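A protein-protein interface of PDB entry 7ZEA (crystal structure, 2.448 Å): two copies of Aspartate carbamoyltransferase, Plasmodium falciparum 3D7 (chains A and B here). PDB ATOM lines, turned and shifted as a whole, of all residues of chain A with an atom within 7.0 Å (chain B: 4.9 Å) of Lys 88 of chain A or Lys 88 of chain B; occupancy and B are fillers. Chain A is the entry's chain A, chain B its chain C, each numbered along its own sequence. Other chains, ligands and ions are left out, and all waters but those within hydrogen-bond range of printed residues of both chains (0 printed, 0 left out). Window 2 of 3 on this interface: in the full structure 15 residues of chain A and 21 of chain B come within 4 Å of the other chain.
Of the printed residues of chain B, Val 62 of chain A touches Leu 83 (3.95 Å).
Gly 86 of chain A touches none of the printed residues of chain B.
Printed residues of chain B within 4 Å of Val 89 of chain A: Leu 83.
Of the printed residues of chain B, Leu 90 of chain A touches Leu 83 (3.97 Å).
Val 62 of chain B touches none of the printed residues of chain A.
Printed residues of chain A within 4 Å of Leu 83 of chain B: Val 62, Lys 88, Val 89 and Leu 90.
Lys 88 of chain B touches just one residue of chain A: Lys 88 (3.8 Å).
The nearest printed residue of chain B that does not touch Leu 90 of chain A is Val 89 of chain B (7.0 Å).
The backbone carbonyl oxygen of Ser 87 of chain B lies within hydrogen-bond range of the side-chain amino group of Lys 88 of chain A (3.0 Å).
Lys 88 of chain A touches Leu 83 of chain B, but with the chains exchanged Leu 83 of chain A does not touch Lys 88 of chain B (7.2 Å).
Lys 88 of chain A touches Gly 86 of chain B, but with the chains exchanged Gly 86 of chain A does not touch Lys 88 of chain B (7.7 Å).
Lys 88 of chain B touches its own counterpart, Lys 88 of chain A.
Leu 90 of chain A touches Leu 83 of chain B, but with the chains exchanged Leu 83 of chain A does not touch Leu 90 of chain B (11.3 Å).
Of the 7 pairs that touch across the chains among the printed residues, 1 has its exchanged pair printed and touching as well.
N of Leu 90 of chain A sits at hydrogen-bond distance from O of Phe 63 of chain A, at 3.0 Å.
N of Phe 63 of chain B lies within hydrogen-bond range of O of Lys 88 of chain B (2.9 Å).
The backbone carbonyl oxygen (O) of Ile 82 of chain B sits at hydrogen-bond distance from the backbone NH (N) of Ser 87 of chain B (3.2 Å).
The backbone carbonyl oxygen of Lys 61 of chain B lies within hydrogen-bond range of the backbone NH of Lys 88 of chain B (3.0 Å).
O of Lys 88 of chain A sits at hydrogen-bond distance from N of Phe 63 of chain A, 2.9 Å away.
The side-chain sulfur of Cys 64 of chain A sits close to the backbone carbonyl oxygen of Leu 90 of chain A, 3.8 Å away.
Val 62 of chain A touches Leu 83 of chain B.
Leu 83 of chain B touches Lys 88 of chain A (O to CD, 3.5 Å).
O of Gly 86 of chain B touches NZ of Lys 88 of chain A, 3.8 Å away.
CG of Lys 88 of chain B touches NZ of Lys 88 of chain A, at 3.8 Å.
Val 89 of chain A touches Leu 83 of chain B (O to CD1, 3.9 Å).
Leu 90 of chain A touches Leu 83 of chain B (CB to CD1, 3.97 Å).
Hydrophobic or aromatic side chains of chain B that line the printed part of chain A: Leu 83.
Printed residues of chain A that touch a printed residue of chain B: Val 62, Lys 88, Val 89 and Leu 90.
Among the printed residues, 7 pairs touch across the chains.
Among the printed residues, no Asp or Glu carboxylate lies within 4 Å of a Lys or Arg side-chain nitrogen of the other chain.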
ATOM      1  N   LEU A  58       4.771  25.197   0.370  1.00  0.00           N
ATOM      2  CA  LEU A  58       3.318  24.931   0.381  1.00  0.00           C
ATOM      3  C   LEU A  58       3.038  23.637  -0.377  1.00  0.00           C
ATOM      4  O   LEU A  58       2.655  23.710  -1.541  1.00  0.00           O
ATOM      5  CB  LEU A  58       2.612  26.113  -0.266  1.00  0.00           C
ATOM      6  CG  LEU A  58       1.086  26.099  -0.149  1.00  0.00           C
ATOM      7  CD1 LEU A  58       0.647  26.544   1.228  1.00  0.00           C
ATOM      8  CD2 LEU A  58       0.424  26.947  -1.221  1.00  0.00           C
ATOM      9  N   GLU A  59       3.319  22.486   0.231  1.00  0.00           N
ATOM     10  CA  GLU A  59       2.893  21.164  -0.285  1.00  0.00           C
ATOM     11  C   GLU A  59       1.587  20.853   0.423  1.00  0.00           C
ATOM     12  O   GLU A  59       1.300  21.471   1.420  1.00  0.00           O
ATOM     13  CB  GLU A  59       3.945  20.070  -0.117  1.00  0.00           C
ATOM     14  CG  GLU A  59       4.970  20.279   0.986  1.00  0.00           C
ATOM     15  CD  GLU A  59       6.091  19.240   0.947  1.00  0.00           C
ATOM     16  OE1 GLU A  59       7.037  19.433   1.726  1.00  0.00           O
ATOM     17  OE2 GLU A  59       6.033  18.226   0.127  1.00  0.00           O
ATOM     18  N   ASN A  60       0.796  19.956  -0.094  1.00  0.00           N
ATOM     19  CA  ASN A  60      -0.438  19.498   0.615  1.00  0.00           C
ATOM     20  C   ASN A  60      -1.636  20.297   0.120  1.00  0.00           C
ATOM     21  O   ASN A  60      -2.700  19.892   0.436  1.00  0.00           O
ATOM     22  CB  ASN A  60      -0.285  19.411   2.146  1.00  0.00           C
ATOM     23  CG  ASN A  60       0.451  18.141   2.624  1.00  0.00           C
ATOM     24  OD1 ASN A  60       1.607  17.831   2.262  1.00  0.00           O
ATOM     25  ND2 ASN A  60      -0.221  17.334   3.446  1.00  0.00           N
ATOM     26  N   LYS A  61      -1.478  21.264  -0.776  1.00  0.00           N
ATOM     27  CA  LYS A  61      -2.628  21.933  -1.415  1.00  0.00           C
ATOM     28  C   LYS A  61      -2.909  21.348  -2.801  1.00  0.00           C
ATOM     29  O   LYS A  61      -2.004  20.904  -3.472  1.00  0.00           O
ATOM     30  CB  LYS A  61      -2.379  23.440  -1.422  1.00  0.00           C
ATOM     31  CG  LYS A  61      -2.130  24.021  -0.040  1.00  0.00           C
ATOM     32  CD  LYS A  61      -3.301  23.862   0.883  1.00  0.00           C
ATOM     33  CE  LYS A  61      -3.027  24.101   2.350  1.00  0.00           C
ATOM     34  NZ  LYS A  61      -4.313  24.397   3.035  1.00  0.00           N
ATOM     35  N   VAL A  62      -4.157  21.405  -3.229  1.00  0.00           N
ATOM     36  CA  VAL A  62      -4.608  20.960  -4.581  1.00  0.00           C
ATOM     37  C   VAL A  62      -5.453  22.095  -5.103  1.00  0.00           C
ATOM     38  O   VAL A  62      -6.354  22.503  -4.377  1.00  0.00           O
ATOM     39  CB  VAL A  62      -5.435  19.668  -4.493  1.00  0.00           C
ATOM     40  CG1 VAL A  62      -5.967  19.261  -5.848  1.00  0.00           C
ATOM     41  CG2 VAL A  62      -4.653  18.561  -3.799  1.00  0.00           C
ATOM     42  N   PHE A  63      -5.078  22.663  -6.233  1.00  0.00           N
ATOM     43  CA  PHE A  63      -5.683  23.871  -6.821  1.00  0.00           C
ATOM     44  C   PHE A  63      -6.368  23.417  -8.089  1.00  0.00           C
ATOM     45  O   PHE A  63      -6.042  22.285  -8.632  1.00  0.00           O
ATOM     46  CB  PHE A  63      -4.611  24.905  -7.163  1.00  0.00           C
ATOM     47  CG  PHE A  63      -3.998  25.568  -5.953  1.00  0.00           C
ATOM     48  CD1 PHE A  63      -4.637  26.618  -5.306  1.00  0.00           C
ATOM     49  CD2 PHE A  63      -2.772  25.143  -5.453  1.00  0.00           C
ATOM     50  CE1 PHE A  63      -4.075  27.200  -4.177  1.00  0.00           C
ATOM     51  CE2 PHE A  63      -2.224  25.729  -4.315  1.00  0.00           C
ATOM     52  CZ  PHE A  63      -2.873  26.766  -3.685  1.00  0.00           C
ATOM     53  N   CYS A  64      -7.318  24.246  -8.532  1.00  0.00           N
ATOM     54  CA  CYS A  64      -7.911  24.127  -9.891  1.00  0.00           C
ATOM     55  C   CYS A  64      -7.599  25.438 -10.612  1.00  0.00           C
ATOM     56  O   CYS A  64      -7.744  26.522 -10.009  1.00  0.00           O
ATOM     57  CB  CYS A  64      -9.397  23.826  -9.881  1.00  0.00           C
ATOM     58  SG  CYS A  64     -10.066  23.721 -11.542  1.00  0.00           S
ATOM     59  N   ILE A  82       2.591  26.989  -8.476  1.00  0.00           N
ATOM     60  CA  ILE A  82       1.930  25.938  -7.651  1.00  0.00           C
ATOM     61  C   ILE A  82       2.867  24.757  -7.536  1.00  0.00           C
ATOM     62  O   ILE A  82       3.068  24.262  -6.435  1.00  0.00           O
ATOM     63  CB  ILE A  82       0.565  25.547  -8.245  1.00  0.00           C
ATOM     64  CG1 ILE A  82      -0.418  26.706  -8.186  1.00  0.00           C
ATOM     65  CG2 ILE A  82      -0.010  24.337  -7.521  1.00  0.00           C
ATOM     66  CD1 ILE A  82      -1.573  26.540  -9.154  1.00  0.00           C
ATOM     67  N   LEU A  83       3.433  24.300  -8.647  1.00  0.00           N
ATOM     68  CA  LEU A  83       4.222  23.046  -8.641  1.00  0.00           C
ATOM     69  C   LEU A  83       5.525  23.278  -7.914  1.00  0.00           C
ATOM     70  O   LEU A  83       5.911  22.424  -7.137  1.00  0.00           O
ATOM     71  CB  LEU A  83       4.419  22.562 -10.075  1.00  0.00           C
ATOM     72  CG  LEU A  83       3.120  22.207 -10.806  1.00  0.00           C
ATOM     73  CD1 LEU A  83       3.428  21.954 -12.261  1.00  0.00           C
ATOM     74  CD2 LEU A  83       2.411  21.008 -10.211  1.00  0.00           C
ATOM     75  N   GLY A  86       5.283  22.965  -4.341  1.00  0.00           N
ATOM     76  CA  GLY A  86       5.125  21.560  -3.915  1.00  0.00           C
ATOM     77  C   GLY A  86       3.690  21.087  -3.960  1.00  0.00           C
ATOM     78  O   GLY A  86       3.457  19.928  -3.767  1.00  0.00           O
ATOM     79  N   SER A  87       2.766  21.950  -4.337  1.00  0.00           N
ATOM     80  CA  SER A  87       1.313  21.652  -4.381  1.00  0.00           C
ATOM     81  C   SER A  87       0.958  21.067  -5.736  1.00  0.00           C
ATOM     82  O   SER A  87       1.868  20.742  -6.522  1.00  0.00           O
ATOM     83  CB  SER A  87       0.517  22.875  -3.988  1.00  0.00           C
ATOM     84  OG  SER A  87       0.543  22.947  -2.567  1.00  0.00           O
ATOM     85  N   LYS A  88      -0.306  20.765  -5.932  1.00  0.00           N
ATOM     86  CA  LYS A  88      -0.757  20.077  -7.161  1.00  0.00           C
ATOM     87  C   LYS A  88      -1.869  20.909  -7.785  1.00  0.00           C
ATOM     88  O   LYS A  88      -2.484  21.660  -7.096  1.00  0.00           O
ATOM     89  CB  LYS A  88      -1.248  18.676  -6.852  1.00  0.00           C
ATOM     90  CG  LYS A  88      -0.201  17.707  -6.352  1.00  0.00           C
ATOM     91  CD  LYS A  88      -0.849  16.453  -5.828  1.00  0.00           C
ATOM     92  CE  LYS A  88       0.110  15.498  -5.183  1.00  0.00           C
ATOM     93  NZ  LYS A  88       1.003  14.905  -6.217  1.00  0.00           N
ATOM     94  N   VAL A  89      -2.069  20.743  -9.066  1.00  0.00           N
ATOM     95  CA  VAL A  89      -3.088  21.494  -9.802  1.00  0.00           C
ATOM     96  C   VAL A  89      -3.731  20.543 -10.829  1.00  0.00           C
ATOM     97  O   VAL A  89      -3.050  19.708 -11.485  1.00  0.00           O
ATOM     98  CB  VAL A  89      -2.484  22.760 -10.427  1.00  0.00           C
ATOM     99  CG1 VAL A  89      -1.309  22.459 -11.341  1.00  0.00           C
ATOM    100  CG2 VAL A  89      -3.512  23.538 -11.220  1.00  0.00           C
ATOM    101  N   LEU A  90      -4.999  20.813 -11.012  1.00  0.00           N
ATOM    102  CA  LEU A  90      -5.932  20.205 -11.952  1.00  0.00           C
ATOM    103  C   LEU A  90      -6.325  21.386 -12.855  1.00  0.00           C
ATOM    104  O   LEU A  90      -6.590  22.475 -12.315  1.00  0.00           O
ATOM    105  CB  LEU A  90      -6.875  19.636 -10.875  1.00  0.00           C
ATOM    106  CG  LEU A  90      -8.339  19.426 -11.080  1.00  0.00           C
ATOM    107  CD1 LEU A  90      -8.943  19.435  -9.699  1.00  0.00           C
ATOM    108  CD2 LEU A  90      -8.986  20.457 -11.966  1.00  0.00           C
ATOM    109  N   ASP A 118      -8.616  23.291  -2.798  1.00  0.00           N
ATOM    110  CA  ASP A 118      -8.293  24.282  -1.739  1.00  0.00           C
ATOM    111  C   ASP A 118      -8.397  25.728  -2.234  1.00  0.00           C
ATOM    112  O   ASP A 118      -8.595  26.619  -1.382  1.00  0.00           O
ATOM    113  CB  ASP A 118      -6.916  24.040  -1.174  1.00  0.00           C
ATOM    114  CG  ASP A 118      -6.814  22.660  -0.591  1.00  0.00           C
ATOM    115  OD1 ASP A 118      -7.587  22.378   0.316  1.00  0.00           O
ATOM    116  OD2 ASP A 118      -5.961  21.887  -1.080  1.00  0.00           O
ATOM    117  N   LYS B  61       1.601   6.585  -6.643  1.00  0.00           N
ATOM    118  CA  LYS B  61       0.870   6.026  -7.788  1.00  0.00           C
ATOM    119  C   LYS B  61       0.850   7.094  -8.896  1.00  0.00           C
ATOM    120  O   LYS B  61       0.814   8.277  -8.596  1.00  0.00           O
ATOM    121  CB  LYS B  61      -0.527   5.558  -7.346  1.00  0.00           C
ATOM    122  CG  LYS B  61      -0.663   4.066  -7.088  1.00  0.00           C
ATOM    123  CD  LYS B  61       0.285   3.448  -6.093  1.00  0.00           C
ATOM    124  CE  LYS B  61       0.344   1.971  -6.324  1.00  0.00           C
ATOM    125  NZ  LYS B  61       0.980   1.282  -5.196  1.00  0.00           N
ATOM    126  N   VAL B  62       0.801   6.638 -10.135  1.00  0.00           N
ATOM    127  CA  VAL B  62       0.681   7.508 -11.323  1.00  0.00           C
ATOM    128  C   VAL B  62      -0.473   6.946 -12.117  1.00  0.00           C
ATOM    129  O   VAL B  62      -0.432   5.748 -12.375  1.00  0.00           O
ATOM    130  CB  VAL B  62       1.982   7.505 -12.140  1.00  0.00           C
ATOM    131  CG1 VAL B  62       1.830   8.395 -13.369  1.00  0.00           C
ATOM    132  CG2 VAL B  62       3.173   7.953 -11.297  1.00  0.00           C
ATOM    133  N   PHE B  63      -1.499   7.750 -12.378  1.00  0.00           N
ATOM    134  CA  PHE B  63      -2.738   7.325 -13.063  1.00  0.00           C
ATOM    135  C   PHE B  63      -2.734   8.000 -14.416  1.00  0.00           C
ATOM    136  O   PHE B  63      -1.995   9.007 -14.607  1.00  0.00           O
ATOM    137  CB  PHE B  63      -3.966   7.712 -12.263  1.00  0.00           C
ATOM    138  CG  PHE B  63      -4.138   6.957 -10.971  1.00  0.00           C
ATOM    139  CD1 PHE B  63      -3.665   7.470  -9.798  1.00  0.00           C
ATOM    140  CD2 PHE B  63      -4.782   5.720 -10.938  1.00  0.00           C
ATOM    141  CE1 PHE B  63      -3.830   6.770  -8.609  1.00  0.00           C
ATOM    142  CE2 PHE B  63      -4.902   4.987  -9.761  1.00  0.00           C
ATOM    143  CZ  PHE B  63      -4.436   5.520  -8.591  1.00  0.00           C
ATOM    144  N   ILE B  82      -7.360  11.854  -6.834  1.00  0.00           N
ATOM    145  CA  ILE B  82      -5.980  11.307  -7.020  1.00  0.00           C
ATOM    146  C   ILE B  82      -4.991  12.267  -6.324  1.00  0.00           C
ATOM    147  O   ILE B  82      -4.100  11.797  -5.591  1.00  0.00           O
ATOM    148  CB  ILE B  82      -5.656  11.150  -8.513  1.00  0.00           C
ATOM    149  CG1 ILE B  82      -6.501  10.063  -9.144  1.00  0.00           C
ATOM    150  CG2 ILE B  82      -4.170  10.894  -8.722  1.00  0.00           C
ATOM    151  CD1 ILE B  82      -6.644  10.173 -10.649  1.00  0.00           C
ATOM    152  N   LEU B  83      -5.112  13.566  -6.579  1.00  0.00           N
ATOM    153  CA  LEU B  83      -4.077  14.521  -6.126  1.00  0.00           C
ATOM    154  C   LEU B  83      -4.176  14.657  -4.598  1.00  0.00           C
ATOM    155  O   LEU B  83      -3.139  14.686  -3.940  1.00  0.00           O
ATOM    156  CB  LEU B  83      -4.276  15.843  -6.881  1.00  0.00           C
ATOM    157  CG  LEU B  83      -4.064  15.762  -8.398  1.00  0.00           C
ATOM    158  CD1 LEU B  83      -4.474  17.054  -9.049  1.00  0.00           C
ATOM    159  CD2 LEU B  83      -2.636  15.466  -8.772  1.00  0.00           C
ATOM    160  N   GLY B  86      -2.442  12.044  -2.819  1.00  0.00           N
ATOM    161  CA  GLY B  86      -0.985  12.298  -2.873  1.00  0.00           C
ATOM    162  C   GLY B  86      -0.308  11.654  -4.076  1.00  0.00           C
ATOM    163  O   GLY B  86       0.905  11.734  -4.194  1.00  0.00           O
ATOM    164  N   SER B  87      -1.093  11.059  -4.970  1.00  0.00           N
ATOM    165  CA  SER B  87      -0.632  10.446  -6.230  1.00  0.00           C
ATOM    166  C   SER B  87      -0.612  11.483  -7.349  1.00  0.00           C
ATOM    167  O   SER B  87      -0.746  12.672  -7.068  1.00  0.00           O
ATOM    168  CB  SER B  87      -1.473   9.222  -6.511  1.00  0.00           C
ATOM    169  OG  SER B  87      -0.996   8.166  -5.676  1.00  0.00           O
ATOM    170  N   LYS B  88      -0.304  11.062  -8.561  1.00  0.00           N
ATOM    171  CA  LYS B  88      -0.111  11.979  -9.703  1.00  0.00           C
ATOM    172  C   LYS B  88      -0.929  11.444 -10.870  1.00  0.00           C
ATOM    173  O   LYS B  88      -1.271  10.246 -10.852  1.00  0.00           O
ATOM    174  CB  LYS B  88       1.355  12.054 -10.102  1.00  0.00           C
ATOM    175  CG  LYS B  88       2.261  12.740  -9.101  1.00  0.00           C
ATOM    176  CD  LYS B  88       3.688  12.408  -9.372  1.00  0.00           C
ATOM    177  CE  LYS B  88       4.626  13.019  -8.385  1.00  0.00           C
ATOM    178  NZ  LYS B  88       4.941  14.361  -8.875  1.00  0.00           N
ATOM    179  N   VAL B  89      -1.260  12.294 -11.838  1.00  0.00           N
ATOM    180  CA  VAL B  89      -2.094  11.843 -12.966  1.00  0.00           C
ATOM    181  C   VAL B  89      -1.656  12.573 -14.232  1.00  0.00           C
ATOM    182  O   VAL B  89      -1.345  13.772 -14.194  1.00  0.00           O
ATOM    183  CB  VAL B  89      -3.610  12.005 -12.654  1.00  0.00           C
ATOM    184  CG1 VAL B  89      -3.980  13.406 -12.253  1.00  0.00           C
ATOM    185  CG2 VAL B  89      -4.478  11.551 -13.811  1.00  0.00           C
ATOM    186  N   LEU B  90      -1.689  11.836 -15.336  1.00  0.00           N
ATOM    187  CA  LEU B  90      -1.593  12.402 -16.699  1.00  0.00           C
ATOM    188  C   LEU B  90      -2.967  12.268 -17.352  1.00  0.00           C
ATOM    189  O   LEU B  90      -3.649  11.250 -17.122  1.00  0.00           O
ATOM    190  CB  LEU B  90      -0.517  11.726 -17.553  1.00  0.00           C
ATOM    191  CG  LEU B  90      -0.463  10.204 -17.656  1.00  0.00           C
ATOM    192  CD1 LEU B  90      -0.295   9.782 -19.089  1.00  0.00           C
ATOM    193  CD2 LEU B  90       0.717   9.682 -16.854  1.00  0.00           C
